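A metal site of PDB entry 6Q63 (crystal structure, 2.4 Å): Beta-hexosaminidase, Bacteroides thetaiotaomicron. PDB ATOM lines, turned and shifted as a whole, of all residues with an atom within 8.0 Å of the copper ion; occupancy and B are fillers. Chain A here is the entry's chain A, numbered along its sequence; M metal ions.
Of the 22 residues printed, 4 come within 4 Å of the copper ion. Along chain A the residues within 4 Å of the copper ion span positions 282 to 345.
The copper ion is bound by SG of Cys 342, SG of Cys 345, SG of Cys 301 and SG of Cys 282.
The side-chain sulfur of Cys 342 lies close to the backbone NH of Lys 344 (3.6 Å). The backbone NH (N) of Ala 302 sits close to the side-chain sulfur (SG) of Cys 345, at 3.6 Å. The side-chain sulfur (SG) of Cys 345 lies close to the backbone NH (N) of Gly 303 (3.5 Å). The side-chain sulfur (SG) of Cys 301 lies close to the backbone NH (N) of Gly 303, at 3.7 Å. The side-chain sulfur (SG) of Cys 301 sits close to the backbone NH (N) of Asn 304 (3.7 Å). The backbone NH of Cys 301 sits at hydrogen-bond distance from the backbone carbonyl oxygen of Leu 280 (2.8 Å).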
ATOM      1  N   GLU A 279     -19.035  -4.848  16.014  1.00  0.00           N
ATOM      2  CA  GLU A 279     -19.856  -5.660  15.074  1.00  0.00           C
ATOM      3  C   GLU A 279     -21.286  -5.837  15.626  1.00  0.00           C
ATOM      4  O   GLU A 279     -22.182  -6.136  14.820  1.00  0.00           O
ATOM      5  CB  GLU A 279     -19.174  -7.014  14.796  1.00  0.00           C
ATOM      6  CG  GLU A 279     -19.042  -7.916  16.016  1.00  0.00           C
ATOM      7  CD  GLU A 279     -17.650  -7.985  16.637  1.00  0.00           C
ATOM      8  OE1 GLU A 279     -17.012  -6.911  16.813  1.00  0.00           O
ATOM      9  OE2 GLU A 279     -17.213  -9.113  16.956  1.00  0.00           O
ATOM     10  N   LEU A 280     -21.497  -5.639  16.933  1.00  0.00           N
ATOM     11  CA  LEU A 280     -22.816  -5.798  17.601  1.00  0.00           C
ATOM     12  C   LEU A 280     -23.721  -4.591  17.307  1.00  0.00           C
ATOM     13  O   LEU A 280     -24.922  -4.680  17.622  1.00  0.00           O
ATOM     14  CB  LEU A 280     -22.606  -5.946  19.114  1.00  0.00           C
ATOM     15  CG  LEU A 280     -21.715  -7.102  19.569  1.00  0.00           C
ATOM     16  CD1 LEU A 280     -21.569  -7.102  21.083  1.00  0.00           C
ATOM     17  CD2 LEU A 280     -22.258  -8.442  19.098  1.00  0.00           C
ATOM     18  N   GLY A 281     -23.171  -3.513  16.747  1.00  0.00           N
ATOM     19  CA  GLY A 281     -23.908  -2.286  16.394  1.00  0.00           C
ATOM     20  C   GLY A 281     -24.308  -2.262  14.932  1.00  0.00           C
ATOM     21  O   GLY A 281     -23.677  -2.987  14.139  1.00  0.00           O
ATOM     22  N   CYS A 282     -25.296  -1.430  14.583  1.00  0.00           N
ATOM     23  CA  CYS A 282     -25.896  -1.330  13.221  1.00  0.00           C
ATOM     24  C   CYS A 282     -24.871  -0.774  12.226  1.00  0.00           C
ATOM     25  O   CYS A 282     -24.675  -1.407  11.168  1.00  0.00           O
ATOM     26  CB  CYS A 282     -27.158  -0.475  13.243  1.00  0.00           C
ATOM     27  SG  CYS A 282     -28.508  -1.188  14.215  1.00  0.00           S
ATOM     28  N   THR A 283     -24.243   0.357  12.535  1.00  0.00           N
ATOM     29  CA  THR A 283     -23.267   1.060  11.655  1.00  0.00           C
ATOM     30  C   THR A 283     -21.941   0.291  11.618  1.00  0.00           C
ATOM     31  O   THR A 283     -21.238   0.381  10.597  1.00  0.00           O
ATOM     32  CB  THR A 283     -23.022   2.513  12.092  1.00  0.00           C
ATOM     33  OG1 THR A 283     -22.260   2.492  13.301  1.00  0.00           O
ATOM     34  CG2 THR A 283     -24.288   3.308  12.294  1.00  0.00           C
ATOM     35  N   VAL A 299     -27.167   1.441  19.552  1.00  0.00           N
ATOM     36  CA  VAL A 299     -27.723   0.328  20.378  1.00  0.00           C
ATOM     37  C   VAL A 299     -27.362  -0.997  19.704  1.00  0.00           C
ATOM     38  O   VAL A 299     -26.825  -0.960  18.575  1.00  0.00           O
ATOM     39  CB  VAL A 299     -29.246   0.502  20.559  1.00  0.00           C
ATOM     40  CG1 VAL A 299     -29.575   1.839  21.203  1.00  0.00           C
ATOM     41  CG2 VAL A 299     -30.008   0.345  19.249  1.00  0.00           C
ATOM     42  N   LEU A 300     -27.645  -2.119  20.368  1.00  0.00           N
ATOM     43  CA  LEU A 300     -27.430  -3.475  19.816  1.00  0.00           C
ATOM     44  C   LEU A 300     -28.279  -3.630  18.544  1.00  0.00           C
ATOM     45  O   LEU A 300     -29.416  -3.130  18.536  1.00  0.00           O
ATOM     46  CB  LEU A 300     -27.817  -4.525  20.865  1.00  0.00           C
ATOM     47  CG  LEU A 300     -26.857  -4.657  22.049  1.00  0.00           C
ATOM     48  CD1 LEU A 300     -27.323  -5.762  22.987  1.00  0.00           C
ATOM     49  CD2 LEU A 300     -25.437  -4.914  21.573  1.00  0.00           C
ATOM     50  N   CYS A 301     -27.715  -4.285  17.528  1.00  0.00           N
ATOM     51  CA  CYS A 301     -28.377  -4.563  16.220  1.00  0.00           C
ATOM     52  C   CYS A 301     -29.247  -5.810  16.340  1.00  0.00           C
ATOM     53  O   CYS A 301     -28.689  -6.926  16.365  1.00  0.00           O
ATOM     54  CB  CYS A 301     -27.337  -4.722  15.118  1.00  0.00           C
ATOM     55  SG  CYS A 301     -28.058  -5.059  13.479  1.00  0.00           S
ATOM     56  N   ALA A 302     -30.578  -5.630  16.414  1.00  0.00           N
ATOM     57  CA  ALA A 302     -31.581  -6.711  16.538  1.00  0.00           C
ATOM     58  C   ALA A 302     -31.545  -7.643  15.318  1.00  0.00           C
ATOM     59  O   ALA A 302     -31.969  -8.801  15.456  1.00  0.00           O
ATOM     60  CB  ALA A 302     -32.960  -6.120  16.736  1.00  0.00           C
ATOM     61  N   GLY A 303     -31.068  -7.153  14.168  1.00  0.00           N
ATOM     62  CA  GLY A 303     -31.008  -7.887  12.892  1.00  0.00           C
ATOM     63  C   GLY A 303     -29.770  -8.775  12.786  1.00  0.00           C
ATOM     64  O   GLY A 303     -29.681  -9.539  11.804  1.00  0.00           O
ATOM     65  N   ASN A 304     -28.870  -8.699  13.773  1.00  0.00           N
ATOM     66  CA  ASN A 304     -27.568  -9.424  13.788  1.00  0.00           C
ATOM     67  C   ASN A 304     -27.706 -10.660  14.673  1.00  0.00           C
ATOM     68  O   ASN A 304     -28.008 -10.500  15.863  1.00  0.00           O
ATOM     69  CB  ASN A 304     -26.446  -8.484  14.257  1.00  0.00           C
ATOM     70  CG  ASN A 304     -25.056  -9.054  14.081  1.00  0.00           C
ATOM     71  OD1 ASN A 304     -24.882 -10.251  13.899  1.00  0.00           O
ATOM     72  ND2 ASN A 304     -24.051  -8.189  14.134  1.00  0.00           N
ATOM     73  N   VAL A 307     -25.591 -10.742  17.862  1.00  0.00           N
ATOM     74  CA  VAL A 307     -26.138  -9.963  19.020  1.00  0.00           C
ATOM     75  C   VAL A 307     -26.954 -10.890  19.931  1.00  0.00           C
ATOM     76  O   VAL A 307     -26.801 -10.804  21.160  1.00  0.00           O
ATOM     77  CB  VAL A 307     -26.958  -8.746  18.549  1.00  0.00           C
ATOM     78  CG1 VAL A 307     -27.893  -8.227  19.624  1.00  0.00           C
ATOM     79  CG2 VAL A 307     -26.048  -7.636  18.037  1.00  0.00           C
ATOM     80  N   ARG A 338     -31.508   4.096  14.606  1.00  0.00           N
ATOM     81  CA  ARG A 338     -30.506   3.241  13.914  1.00  0.00           C
ATOM     82  C   ARG A 338     -31.222   2.065  13.217  1.00  0.00           C
ATOM     83  O   ARG A 338     -30.886   1.787  12.044  1.00  0.00           O
ATOM     84  CB  ARG A 338     -29.434   2.716  14.867  1.00  0.00           C
ATOM     85  CG  ARG A 338     -28.419   3.750  15.317  1.00  0.00           C
ATOM     86  CD  ARG A 338     -27.564   4.339  14.195  1.00  0.00           C
ATOM     87  NE  ARG A 338     -26.713   5.375  14.767  1.00  0.00           N
ATOM     88  CZ  ARG A 338     -27.049   6.650  14.932  1.00  0.00           C
ATOM     89  NH1 ARG A 338     -28.227   7.100  14.528  1.00  0.00           N
ATOM     90  NH2 ARG A 338     -26.194   7.488  15.495  1.00  0.00           N
ATOM     91  N   TRP A 339     -32.175   1.439  13.915  1.00  0.00           N
ATOM     92  CA  TRP A 339     -32.982   0.284  13.441  1.00  0.00           C
ATOM     93  C   TRP A 339     -33.740   0.654  12.164  1.00  0.00           C
ATOM     94  O   TRP A 339     -33.820  -0.203  11.266  1.00  0.00           O
ATOM     95  CB  TRP A 339     -33.933  -0.201  14.536  1.00  0.00           C
ATOM     96  CG  TRP A 339     -33.253  -0.926  15.660  1.00  0.00           C
ATOM     97  CD1 TRP A 339     -31.908  -1.089  15.828  1.00  0.00           C
ATOM     98  CD2 TRP A 339     -33.877  -1.554  16.789  1.00  0.00           C
ATOM     99  NE1 TRP A 339     -31.659  -1.790  16.976  1.00  0.00           N
ATOM    100  CE2 TRP A 339     -32.847  -2.087  17.594  1.00  0.00           C
ATOM    101  CE3 TRP A 339     -35.205  -1.725  17.204  1.00  0.00           C
ATOM    102  CZ2 TRP A 339     -33.098  -2.781  18.771  1.00  0.00           C
ATOM    103  CZ3 TRP A 339     -35.453  -2.405  18.380  1.00  0.00           C
ATOM    104  CH2 TRP A 339     -34.415  -2.918  19.155  1.00  0.00           C
ATOM    105  N   GLU A 340     -34.272   1.879  12.084  1.00  0.00           N
ATOM    106  CA  GLU A 340     -35.059   2.398  10.933  1.00  0.00           C
ATOM    107  C   GLU A 340     -34.193   2.418   9.663  1.00  0.00           C
ATOM    108  O   GLU A 340     -34.759   2.202   8.570  1.00  0.00           O
ATOM    109  CB  GLU A 340     -35.567   3.816  11.225  1.00  0.00           C
ATOM    110  CG  GLU A 340     -36.709   3.846  12.230  1.00  0.00           C
ATOM    111  CD  GLU A 340     -37.022   5.222  12.814  1.00  0.00           C
ATOM    112  OE1 GLU A 340     -36.494   6.226  12.303  1.00  0.00           O
ATOM    113  OE2 GLU A 340     -37.786   5.263  13.796  1.00  0.00           O
ATOM    114  N   LYS A 341     -32.883   2.644   9.798  1.00  0.00           N
ATOM    115  CA  LYS A 341     -31.920   2.869   8.677  1.00  0.00           C
ATOM    116  C   LYS A 341     -31.089   1.616   8.402  1.00  0.00           C
ATOM    117  O   LYS A 341     -30.379   1.603   7.377  1.00  0.00           O
ATOM    118  CB  LYS A 341     -30.995   4.048   9.012  1.00  0.00           C
ATOM    119  CG  LYS A 341     -31.663   5.414   9.058  1.00  0.00           C
ATOM    120  CD  LYS A 341     -32.458   5.735   7.800  1.00  0.00           C
ATOM    121  CE  LYS A 341     -32.790   7.206   7.656  1.00  0.00           C
ATOM    122  NZ  LYS A 341     -33.682   7.677   8.736  1.00  0.00           N
ATOM    123  N   CYS A 342     -31.159   0.611   9.275  1.00  0.00           N
ATOM    124  CA  CYS A 342     -30.284  -0.596   9.269  1.00  0.00           C
ATOM    125  C   CYS A 342     -30.890  -1.675   8.363  1.00  0.00           C
ATOM    126  O   CYS A 342     -31.985  -2.158   8.621  1.00  0.00           O
ATOM    127  CB  CYS A 342     -30.106  -1.125  10.696  1.00  0.00           C
ATOM    128  SG  CYS A 342     -29.151  -2.657  10.790  1.00  0.00           S
ATOM    129  N   PRO A 343     -30.187  -2.075   7.268  1.00  0.00           N
ATOM    130  CA  PRO A 343     -30.688  -3.129   6.386  1.00  0.00           C
ATOM    131  C   PRO A 343     -30.952  -4.475   7.087  1.00  0.00           C
ATOM    132  O   PRO A 343     -31.870  -5.161   6.669  1.00  0.00           O
ATOM    133  CB  PRO A 343     -29.582  -3.334   5.333  1.00  0.00           C
ATOM    134  CG  PRO A 343     -28.664  -2.137   5.455  1.00  0.00           C
ATOM    135  CD  PRO A 343     -28.907  -1.520   6.822  1.00  0.00           C
ATOM    136  N   LYS A 344     -30.159  -4.831   8.091  1.00  0.00           N
ATOM    137  CA  LYS A 344     -30.283  -6.118   8.830  1.00  0.00           C
ATOM    138  C   LYS A 344     -31.544  -6.104   9.690  1.00  0.00           C
ATOM    139  O   LYS A 344     -32.296  -7.086   9.650  1.00  0.00           O
ATOM    140  CB  LYS A 344     -29.060  -6.377   9.716  1.00  0.00           C
ATOM    141  CG  LYS A 344     -27.705  -6.382   9.002  1.00  0.00           C
ATOM    142  CD  LYS A 344     -26.553  -6.453   9.963  1.00  0.00           C
ATOM    143  CE  LYS A 344     -25.200  -6.310   9.293  1.00  0.00           C
ATOM    144  NZ  LYS A 344     -24.098  -6.462  10.269  1.00  0.00           N
ATOM    145  N   CYS A 345     -31.756  -5.035  10.477  1.00  0.00           N
ATOM    146  CA  CYS A 345     -32.939  -4.852  11.359  1.00  0.00           C
ATOM    147  C   CYS A 345     -34.223  -4.817  10.509  1.00  0.00           C
ATOM    148  O   CYS A 345     -35.227  -5.415  10.938  1.00  0.00           O
ATOM    149  CB  CYS A 345     -32.798  -3.609  12.232  1.00  0.00           C
ATOM    150  SG  CYS A 345     -31.503  -3.746  13.494  1.00  0.00           S
ATOM    151  N   GLN A 346     -34.187  -4.169   9.342  1.00  0.00           N
ATOM    152  CA  GLN A 346     -35.344  -4.074   8.416  1.00  0.00           C
ATOM    153  C   GLN A 346     -35.630  -5.441   7.783  1.00  0.00           C
ATOM    154  O   GLN A 346     -36.816  -5.738   7.534  1.00  0.00           O
ATOM    155  CB  GLN A 346     -35.120  -2.997   7.351  1.00  0.00           C
ATOM    156  CG  GLN A 346     -35.132  -1.577   7.904  1.00  0.00           C
ATOM    157  CD  GLN A 346     -36.410  -1.234   8.627  1.00  0.00           C
ATOM    158  OE1 GLN A 346     -37.505  -1.452   8.119  1.00  0.00           O
ATOM    159  NE2 GLN A 346     -36.271  -0.699   9.828  1.00  0.00           N
ATOM    160  N   LEU A 366     -40.056  -4.916  16.840  1.00  0.00           N
ATOM    161  CA  LEU A 366     -38.683  -5.465  16.769  1.00  0.00           C
ATOM    162  C   LEU A 366     -38.053  -5.506  18.163  1.00  0.00           C
ATOM    163  O   LEU A 366     -37.305  -6.468  18.438  1.00  0.00           O
ATOM    164  CB  LEU A 366     -37.821  -4.632  15.800  1.00  0.00           C
ATOM    165  CG  LEU A 366     -36.397  -5.146  15.599  1.00  0.00           C
ATOM    166  CD1 LEU A 366     -36.389  -6.606  15.185  1.00  0.00           C
ATOM    167  CD2 LEU A 366     -35.652  -4.299  14.577  1.00  0.00           C
HETATM  168 CU    CU M   1     -29.284  -3.093  12.992  1.00  0.00          CU
